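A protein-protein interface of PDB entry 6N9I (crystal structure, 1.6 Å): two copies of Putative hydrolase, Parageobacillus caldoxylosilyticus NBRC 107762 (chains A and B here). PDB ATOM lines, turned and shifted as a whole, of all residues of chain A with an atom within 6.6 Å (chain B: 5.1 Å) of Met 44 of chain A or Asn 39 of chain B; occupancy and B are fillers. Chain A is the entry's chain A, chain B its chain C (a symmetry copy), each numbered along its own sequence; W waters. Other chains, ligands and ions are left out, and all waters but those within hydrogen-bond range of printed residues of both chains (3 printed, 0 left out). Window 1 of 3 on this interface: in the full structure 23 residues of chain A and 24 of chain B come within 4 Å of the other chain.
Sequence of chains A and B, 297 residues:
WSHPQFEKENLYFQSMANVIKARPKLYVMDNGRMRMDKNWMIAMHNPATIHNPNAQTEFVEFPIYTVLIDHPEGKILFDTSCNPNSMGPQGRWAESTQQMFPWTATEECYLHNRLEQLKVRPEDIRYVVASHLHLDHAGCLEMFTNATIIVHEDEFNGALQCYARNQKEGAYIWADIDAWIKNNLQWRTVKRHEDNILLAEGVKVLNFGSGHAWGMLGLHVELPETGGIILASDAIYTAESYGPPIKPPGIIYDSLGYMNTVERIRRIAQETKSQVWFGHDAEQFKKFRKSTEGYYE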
ATOM      1  N   LYS A  38      10.910  -5.301 -14.996  1.00  0.00           N
ATOM      2  CA  LYS A  38      11.429  -6.242 -15.979  1.00  0.00           C
ATOM      3  C   LYS A  38      10.337  -6.577 -17.001  1.00  0.00           C
ATOM      4  O   LYS A  38      10.637  -7.093 -18.077  1.00  0.00           O
ATOM      5  CB  LYS A  38      11.957  -7.520 -15.320  1.00  0.00           C
ATOM      6  CG  LYS A  38      12.730  -8.435 -16.263  1.00  0.00           C
ATOM      7  CD  LYS A  38      13.095  -9.775 -15.664  1.00  0.00           C
ATOM      8  CE  LYS A  38      13.561 -10.777 -16.700  1.00  0.00           C
ATOM      9  NZ  LYS A  38      14.951 -10.513 -17.143  1.00  0.00           N
ATOM     10  N   ASN A  39       9.074  -6.292 -16.660  1.00  0.00           N
ATOM     11  CA  ASN A  39       7.978  -6.488 -17.605  1.00  0.00           C
ATOM     12  C   ASN A  39       8.154  -5.548 -18.804  1.00  0.00           C
ATOM     13  O   ASN A  39       7.777  -5.899 -19.921  1.00  0.00           O
ATOM     14  CB  ASN A  39       6.609  -6.304 -16.944  1.00  0.00           C
ATOM     15  CG  ASN A  39       6.153  -7.529 -16.177  1.00  0.00           C
ATOM     16  OD1 ASN A  39       5.621  -7.415 -15.075  1.00  0.00           O
ATOM     17  ND2 ASN A  39       6.358  -8.707 -16.747  1.00  0.00           N
ATOM     18  N   ILE A  42      10.900  -7.573 -20.760  1.00  0.00           N
ATOM     19  CA  ILE A  42      10.361  -8.843 -21.238  1.00  0.00           C
ATOM     20  C   ILE A  42       8.890  -8.935 -20.818  1.00  0.00           C
ATOM     21  O   ILE A  42       8.586  -9.185 -19.650  1.00  0.00           O
ATOM     22  CB  ILE A  42      11.173 -10.031 -20.684  1.00  0.00           C
ATOM     23  CG1 ILE A  42      12.677  -9.852 -20.902  1.00  0.00           C
ATOM     24  CG2 ILE A  42      10.671 -11.342 -21.271  1.00  0.00           C
ATOM     25  CD1 ILE A  42      13.115 -10.002 -22.342  1.00  0.00           C
ATOM     26  N   ALA A  43       7.984  -8.736 -21.780  1.00  0.00           N
ATOM     27  CA  ALA A  43       6.546  -8.698 -21.504  1.00  0.00           C
ATOM     28  C   ALA A  43       6.085 -10.031 -20.902  1.00  0.00           C
ATOM     29  O   ALA A  43       6.442 -11.101 -21.392  1.00  0.00           O
ATOM     30  CB  ALA A  43       5.783  -8.374 -22.766  1.00  0.00           C
ATOM     31  N   MET A  44       5.285  -9.936 -19.836  1.00  0.00           N
ATOM     32  CA  MET A  44       4.656 -11.085 -19.184  1.00  0.00           C
ATOM     33  C   MET A  44       5.703 -12.156 -18.857  1.00  0.00           C
ATOM     34  O   MET A  44       5.498 -13.330 -19.149  1.00  0.00           O
ATOM     35  CB  MET A  44       3.583 -11.702 -20.088  1.00  0.00           C
ATOM     36  CG  MET A  44       2.445 -10.755 -20.428  1.00  0.00           C
ATOM     37  SD  MET A  44       1.601 -10.093 -18.968  1.00  0.00           S
ATOM     38  CE  MET A  44       1.256 -11.602 -18.063  1.00  0.00           C
ATOM     39  N   HIS A  45       6.807 -11.745 -18.226  1.00  0.00           N
ATOM     40  CA  HIS A  45       7.922 -12.647 -17.944  1.00  0.00           C
ATOM     41  C   HIS A  45       7.538 -13.660 -16.858  1.00  0.00           C
ATOM     42  O   HIS A  45       8.017 -14.792 -16.873  1.00  0.00           O
ATOM     43  CB  HIS A  45       9.184 -11.855 -17.571  1.00  0.00           C
ATOM     44  CG  HIS A  45       9.128 -11.204 -16.230  1.00  0.00           C
ATOM     45  ND1 HIS A  45       9.629 -11.808 -15.092  1.00  0.00           N
ATOM     46  CD2 HIS A  45       8.651 -10.000 -15.842  1.00  0.00           C
ATOM     47  CE1 HIS A  45       9.454 -11.007 -14.059  1.00  0.00           C
ATOM     48  NE2 HIS A  45       8.857  -9.891 -14.493  1.00  0.00           N
ATOM     49  N   ASN A  46       6.675 -13.248 -15.922  1.00  0.00           N
ATOM     50  CA  ASN A  46       6.312 -14.083 -14.774  1.00  0.00           C
ATOM     51  C   ASN A  46       4.807 -14.007 -14.526  1.00  0.00           C
ATOM     52  O   ASN A  46       4.363 -13.411 -13.547  1.00  0.00           O
ATOM     53  CB  ASN A  46       7.090 -13.677 -13.520  1.00  0.00           C
ATOM     54  CG  ASN A  46       6.792 -14.562 -12.329  1.00  0.00           C
ATOM     55  OD1 ASN A  46       6.558 -15.760 -12.483  1.00  0.00           O
ATOM     56  ND2 ASN A  46       6.799 -13.985 -11.138  1.00  0.00           N
ATOM     57  N   PRO A  47       3.982 -14.635 -15.392  1.00  0.00           N
ATOM     58  CA  PRO A  47       2.524 -14.538 -15.291  1.00  0.00           C
ATOM     59  C   PRO A  47       1.946 -15.190 -14.028  1.00  0.00           C
ATOM     60  O   PRO A  47       2.394 -16.262 -13.619  1.00  0.00           O
ATOM     61  CB  PRO A  47       2.009 -15.291 -16.530  1.00  0.00           C
ATOM     62  CG  PRO A  47       3.209 -15.394 -17.454  1.00  0.00           C
ATOM     63  CD  PRO A  47       4.410 -15.454 -16.535  1.00  0.00           C
ATOM     64  N   ALA A  48       0.941 -14.535 -13.440  1.00  0.00           N
ATOM     65  CA  ALA A  48       0.221 -15.070 -12.295  1.00  0.00           C
ATOM     66  C   ALA A  48      -0.439 -16.396 -12.686  1.00  0.00           C
ATOM     67  O   ALA A  48      -0.870 -16.575 -13.828  1.00  0.00           O
ATOM     68  CB  ALA A  48      -0.801 -14.072 -11.810  1.00  0.00           C
ATOM     69  N   ALA A  55       1.770 -12.952  -8.325  1.00  0.00           N
ATOM     70  CA  ALA A  55       3.137 -12.949  -8.831  1.00  0.00           C
ATOM     71  C   ALA A  55       3.692 -11.520  -8.818  1.00  0.00           C
ATOM     72  O   ALA A  55       3.016 -10.576  -9.233  1.00  0.00           O
ATOM     73  CB  ALA A  55       3.175 -13.536 -10.219  1.00  0.00           C
ATOM     74  N   PRO A 248       9.137 -10.423 -26.886  1.00  0.00           N
ATOM     75  CA  PRO A 248       8.974  -8.982 -27.072  1.00  0.00           C
ATOM     76  C   PRO A 248       8.870  -8.199 -25.768  1.00  0.00           C
ATOM     77  O   PRO A 248       8.573  -8.756 -24.713  1.00  0.00           O
ATOM     78  CB  PRO A 248       7.676  -8.860 -27.884  1.00  0.00           C
ATOM     79  CG  PRO A 248       6.920 -10.141 -27.599  1.00  0.00           C
ATOM     80  CD  PRO A 248       7.978 -11.194 -27.355  1.00  0.00           C
ATOM     81  N   GLY A 250       7.558  -4.983 -23.063  1.00  0.00           N
ATOM     82  CA  GLY A 250       6.359  -4.279 -22.630  1.00  0.00           C
ATOM     83  C   GLY A 250       6.293  -2.885 -23.233  1.00  0.00           C
ATOM     84  O   GLY A 250       5.208  -2.375 -23.514  1.00  0.00           O
ATOM     85  N   ASP B  37      -4.014 -13.406 -14.833  1.00  0.00           N
ATOM     86  CA  ASP B  37      -3.191 -12.253 -14.506  1.00  0.00           C
ATOM     87  C   ASP B  37      -3.820 -11.011 -15.143  1.00  0.00           C
ATOM     88  O   ASP B  37      -4.125 -11.016 -16.336  1.00  0.00           O
ATOM     89  CB  ASP B  37      -1.762 -12.476 -15.008  1.00  0.00           C
ATOM     90  CG  ASP B  37      -0.749 -11.463 -14.504  1.00  0.00           C
ATOM     91  OD1 ASP B  37      -1.120 -10.280 -14.365  1.00  0.00           O
ATOM     92  OD2 ASP B  37       0.410 -11.871 -14.260  1.00  0.00           O
ATOM     93  N   LYS B  38      -4.017  -9.953 -14.348  1.00  0.00           N
ATOM     94  CA  LYS B  38      -4.663  -8.751 -14.865  1.00  0.00           C
ATOM     95  C   LYS B  38      -3.802  -8.131 -15.971  1.00  0.00           C
ATOM     96  O   LYS B  38      -4.302  -7.362 -16.786  1.00  0.00           O
ATOM     97  CB  LYS B  38      -4.926  -7.700 -13.782  1.00  0.00           C
ATOM     98  CG  LYS B  38      -5.932  -6.644 -14.223  1.00  0.00           C
ATOM     99  CD  LYS B  38      -6.121  -5.477 -13.285  1.00  0.00           C
ATOM    100  CE  LYS B  38      -7.102  -4.469 -13.849  1.00  0.00           C
ATOM    101  NZ  LYS B  38      -7.483  -3.438 -12.855  1.00  0.00           N
ATOM    102  N   ASN B  39      -2.508  -8.463 -15.984  1.00  0.00           N
ATOM    103  CA  ASN B  39      -1.590  -7.906 -16.976  1.00  0.00           C
ATOM    104  C   ASN B  39      -1.942  -8.438 -18.371  1.00  0.00           C
ATOM    105  O   ASN B  39      -1.687  -7.763 -19.366  1.00  0.00           O
ATOM    106  CB  ASN B  39      -0.128  -8.170 -16.617  1.00  0.00           C
ATOM    107  CG  ASN B  39       0.403  -7.197 -15.585  1.00  0.00           C
ATOM    108  OD1 ASN B  39       0.115  -6.001 -15.643  1.00  0.00           O
ATOM    109  ND2 ASN B  39       1.181  -7.698 -14.639  1.00  0.00           N
ATOM    110  N   TRP B  40      -2.526  -9.641 -18.441  1.00  0.00           N
ATOM    111  CA  TRP B  40      -3.046 -10.161 -19.707  1.00  0.00           C
ATOM    112  C   TRP B  40      -4.156  -9.231 -20.207  1.00  0.00           C
ATOM    113  O   TRP B  40      -4.245  -8.937 -21.391  1.00  0.00           O
ATOM    114  CB  TRP B  40      -3.607 -11.582 -19.574  1.00  0.00           C
ATOM    115  CG  TRP B  40      -2.629 -12.681 -19.285  1.00  0.00           C
ATOM    116  CD1 TRP B  40      -2.688 -13.558 -18.241  1.00  0.00           C
ATOM    117  CD2 TRP B  40      -1.492 -13.076 -20.073  1.00  0.00           C
ATOM    118  NE1 TRP B  40      -1.655 -14.451 -18.307  1.00  0.00           N
ATOM    119  CE2 TRP B  40      -0.904 -14.180 -19.419  1.00  0.00           C
ATOM    120  CE3 TRP B  40      -0.903 -12.598 -21.248  1.00  0.00           C
ATOM    121  CZ2 TRP B  40       0.240 -14.811 -19.905  1.00  0.00           C
ATOM    122  CZ3 TRP B  40       0.228 -13.222 -21.727  1.00  0.00           C
ATOM    123  CH2 TRP B  40       0.790 -14.312 -21.063  1.00  0.00           C
ATOM    124  N   MET B  41      -5.005  -8.785 -19.275  1.00  0.00           N
ATOM    125  CA  MET B  41      -6.194  -8.011 -19.606  1.00  0.00           C
ATOM    126  C   MET B  41      -5.821  -6.545 -19.853  1.00  0.00           C
ATOM    127  O   MET B  41      -6.292  -5.941 -20.816  1.00  0.00           O
ATOM    128  CB  MET B  41      -7.231  -8.091 -18.482  1.00  0.00           C
ATOM    129  CG  MET B  41      -8.514  -7.354 -18.803  1.00  0.00           C
ATOM    130  SD  MET B  41      -9.786  -7.603 -17.544  1.00  0.00           S
ATOM    131  CE  MET B  41     -10.210  -9.320 -17.832  1.00  0.00           C
ATOM    132  N   ILE B  42      -4.988  -5.988 -18.965  1.00  0.00           N
ATOM    133  CA  ILE B  42      -4.548  -4.601 -19.049  1.00  0.00           C
ATOM    134  C   ILE B  42      -3.020  -4.570 -18.940  1.00  0.00           C
ATOM    135  O   ILE B  42      -2.473  -4.684 -17.846  1.00  0.00           O
ATOM    136  CB  ILE B  42      -5.201  -3.751 -17.940  1.00  0.00           C
ATOM    137  CG1 ILE B  42      -6.726  -3.877 -17.946  1.00  0.00           C
ATOM    138  CG2 ILE B  42      -4.763  -2.298 -18.041  1.00  0.00           C
ATOM    139  CD1 ILE B  42      -7.394  -3.138 -19.078  1.00  0.00           C
ATOM    140  N   ALA B  43      -2.347  -4.415 -20.083  1.00  0.00           N
ATOM    141  CA  ALA B  43      -0.886  -4.453 -20.138  1.00  0.00           C
ATOM    142  C   ALA B  43      -0.295  -3.425 -19.167  1.00  0.00           C
ATOM    143  O   ALA B  43      -0.721  -2.270 -19.138  1.00  0.00           O
ATOM    144  CB  ALA B  43      -0.415  -4.205 -21.550  1.00  0.00           C
ATOM    145  N   MET B  44       0.687  -3.871 -18.375  1.00  0.00           N
ATOM    146  CA  MET B  44       1.461  -3.014 -17.474  1.00  0.00           C
ATOM    147  C   MET B  44       0.524  -2.153 -16.619  1.00  0.00           C
ATOM    148  O   MET B  44       0.719  -0.944 -16.502  1.00  0.00           O
ATOM    149  CB  MET B  44       2.393  -2.098 -18.273  1.00  0.00           C
ATOM    150  CG  MET B  44       3.369  -2.849 -19.156  1.00  0.00           C
ATOM    151  SD  MET B  44       4.484  -3.914 -18.212  1.00  0.00           S
ATOM    152  CE  MET B  44       5.166  -2.733 -17.050  1.00  0.00           C
ATOM    153  N   HIS B  45      -0.476  -2.791 -16.004  1.00  0.00           N
ATOM    154  CA  HIS B  45      -1.523  -2.078 -15.275  1.00  0.00           C
ATOM    155  C   HIS B  45      -0.957  -1.442 -14.000  1.00  0.00           C
ATOM    156  O   HIS B  45      -1.522  -0.475 -13.484  1.00  0.00           O
ATOM    157  CB  HIS B  45      -2.694  -3.017 -14.955  1.00  0.00           C
ATOM    158  CG  HIS B  45      -2.466  -3.887 -13.764  1.00  0.00           C
ATOM    159  ND1 HIS B  45      -1.729  -5.052 -13.832  1.00  0.00           N
ATOM    160  CD2 HIS B  45      -2.881  -3.773 -12.484  1.00  0.00           C
ATOM    161  CE1 HIS B  45      -1.698  -5.618 -12.643  1.00  0.00           C
ATOM    162  NE2 HIS B  45      -2.396  -4.853 -11.797  1.00  0.00           N
ATOM    163  N   ASN B  46       0.154  -1.994 -13.500  1.00  0.00           N
ATOM    164  CA  ASN B  46       0.727  -1.580 -12.222  1.00  0.00           C
ATOM    165  C   ASN B  46       2.246  -1.727 -12.260  1.00  0.00           C
ATOM    166  O   ASN B  46       2.805  -2.610 -11.612  1.00  0.00           O
ATOM    167  CB  ASN B  46       0.141  -2.395 -11.067  1.00  0.00           C
ATOM    168  CG  ASN B  46       0.729  -2.020  -9.724  1.00  0.00           C
ATOM    169  OD1 ASN B  46       1.114  -0.873  -9.510  1.00  0.00           O
ATOM    170  ND2 ASN B  46       0.800  -2.981  -8.816  1.00  0.00           N
ATOM    171  N   THR B  57       1.072  -8.352  -9.077  1.00  0.00           N
ATOM    172  CA  THR B  57      -0.112  -8.285  -9.923  1.00  0.00           C
ATOM    173  C   THR B  57      -1.308  -8.863  -9.162  1.00  0.00           C
ATOM    174  O   THR B  57      -1.209  -9.172  -7.975  1.00  0.00           O
ATOM    175  CB  THR B  57       0.114  -9.023 -11.250  1.00  0.00           C
ATOM    176  OG1 THR B  57      -0.977  -8.732 -12.121  1.00  0.00           O
ATOM    177  CG2 THR B  57       0.237 -10.521 -11.071  1.00  0.00           C
ATOM    178  N   PRO B 249      -4.406  -4.728 -24.171  1.00  0.00           N
ATOM    179  CA  PRO B 249      -4.134  -5.953 -23.423  1.00  0.00           C
ATOM    180  C   PRO B 249      -2.674  -6.419 -23.496  1.00  0.00           C
ATOM    181  O   PRO B 249      -1.910  -5.955 -24.347  1.00  0.00           O
ATOM    182  CB  PRO B 249      -5.044  -6.977 -24.113  1.00  0.00           C
ATOM    183  CG  PRO B 249      -5.142  -6.489 -25.540  1.00  0.00           C
ATOM    184  CD  PRO B 249      -5.084  -4.980 -25.451  1.00  0.00           C
ATOM    185  N   GLY B 250      -2.314  -7.328 -22.585  1.00  0.00           N
ATOM    186  CA  GLY B 250      -1.055  -8.060 -22.653  1.00  0.00           C
ATOM    187  C   GLY B 250      -1.122  -9.165 -23.697  1.00  0.00           C
ATOM    188  O   GLY B 250      -0.120  -9.491 -24.327  1.00  0.00           O
ATOM    189  N   ILE B 251      -2.316  -9.750 -23.861  1.00  0.00           N
ATOM    190  CA  ILE B 251      -2.585 -10.721 -24.924  1.00  0.00           C
ATOM    191  C   ILE B 251      -2.931  -9.952 -26.203  1.00  0.00           C
ATOM    192  O   ILE B 251      -4.052  -9.456 -26.361  1.00  0.00           O
ATOM    193  CB  ILE B 251      -3.718 -11.695 -24.543  1.00  0.00           C
ATOM    194  CG1 ILE B 251      -3.401 -12.477 -23.266  1.00  0.00           C
ATOM    195  CG2 ILE B 251      -4.028 -12.628 -25.705  1.00  0.00           C
ATOM    196  CD1 ILE B 251      -4.435 -13.525 -22.921  1.00  0.00           C
HETATM  197  O   HOH W   1      -2.616 -15.810 -15.811  1.00  0.00           O
HETATM  198  O   HOH W   2       1.633  -6.539 -19.115  1.00  0.00           O
HETATM  199  O   HOH W   3       4.216  -7.379 -19.440  1.00  0.00           O
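O of Ala 55 of chain A is in hydrogen-bond range of N of Thr 57 of chain B (3.0 Å).
The backbone NH (N) of Ala 48 of chain A lies within hydrogen-bond range of the side-chain carboxylate (OD2) of Asp 37 of chain B, at 2.8 Å.
The backbone NH of Met 44 of chain A sits close to the side-chain amide nitrogen of Asn 39 of chain A.
OG1 of Thr 57 of chain B lies within hydrogen-bond range of OD1 of Asp 37 of chain B (2.7 Å).
The backbone NH (N) of Gly 250 of chain B is in hydrogen-bond range of the backbone carbonyl oxygen (O) of Asn 39 of chain B.
ND2 of Asn 39 of chain B is in hydrogen-bond range of OG1 of Thr 57 of chain B, at 3.5 Å.
The backbone NH (N) of Gly 250 of chain B lies within hydrogen-bond range of the backbone carbonyl oxygen (O) of Trp 40 of chain B, at 2.8 Å.
The side-chain amide nitrogen (ND2) of Asn 39 of chain A sits close to the backbone NH (N) of His 45 of chain A (3.4 Å).
Asn 39 of chain A touches Met 44 of chain B (CB to SD, 3.4 Å).
OD2 of Asp 37 of chain B touches CE of Met 44 of chain A, 3.9 Å away.
CB of Asn 39 of chain B touches SD of Met 44 of chain A (3.5 Å).
CG of Met 44 of chain A touches CZ3 of Trp 40 of chain B, at 3.6 Å.
OD2 of Asp 37 of chain B touches CA of Pro 47 of chain A (3.6 Å).
CZ2 of Trp 40 of chain B touches CB of Pro 47 of chain A, 3.8 Å away.
Thr 57 of chain B touches Ala 48 of chain A (CG2 to CB, 3.8 Å).
Met 44 of chain A touches just these residues of chain B: Asp 37, Asn 39 and Trp 40.
Asn 46 of chain A touches none of the printed residues of chain B.
Gly 250 of chain A touches none of the printed residues of chain B.
Printed residues of chain A within 4 Å of Asp 37 of chain B: Met 44, Pro 47 and Ala 48.
Of chain A, only Met 44 (3.5 Å) comes within 4 Å of Asn 39 of chain B.
Of the printed residues of chain A, Met 44 of chain B touches Asn 39.
Printed residues of chain A within 4 Å of Thr 57 of chain B: Ala 48 (3.8 Å) and Ala 55 (3.0 Å).
The nearest residue of chain B that does not touch Met 44 of chain A is Gly 250 of chain B (4.8 Å).
The nearest printed residue of chain A that does not touch Met 44 of chain B is Gly 250 of chain A (4.8 Å).
Of the 14 printed residues of chain B, 5 touch a printed residue of chain A.
Of the 12 printed residues of chain A, 5 touch a printed residue of chain B.
Along chain A the printed residues that touch a printed residue of chain B span positions 39 to 55.
Asn 39 of chain A touches Met 44 of chain B, and with the chains exchanged Met 44 of chain A touches Asn 39 of chain B.
Positions printed for both chains: 38, 39, 42, 43, 44, 45, 46 and 250.
Of the 9 pairs that touch across the chains among the printed residues, 2 have their exchanged pair printed and touching as well.
Water W1 lies within hydrogen-bond range of O of Ala 48 of chain A (2.8 Å), N of Asp 37 of chain B (2.9 Å) and NE1 of Trp 40 of chain B (3.0 Å).
Water W3 lies within hydrogen-bond range of N of Met 44 of chain A (2.8 Å) and SD of Met 44 of chain B (3.7 Å).
Water W2 bridges N of Met 44 of chain B and SD of Met 44 of chain A.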
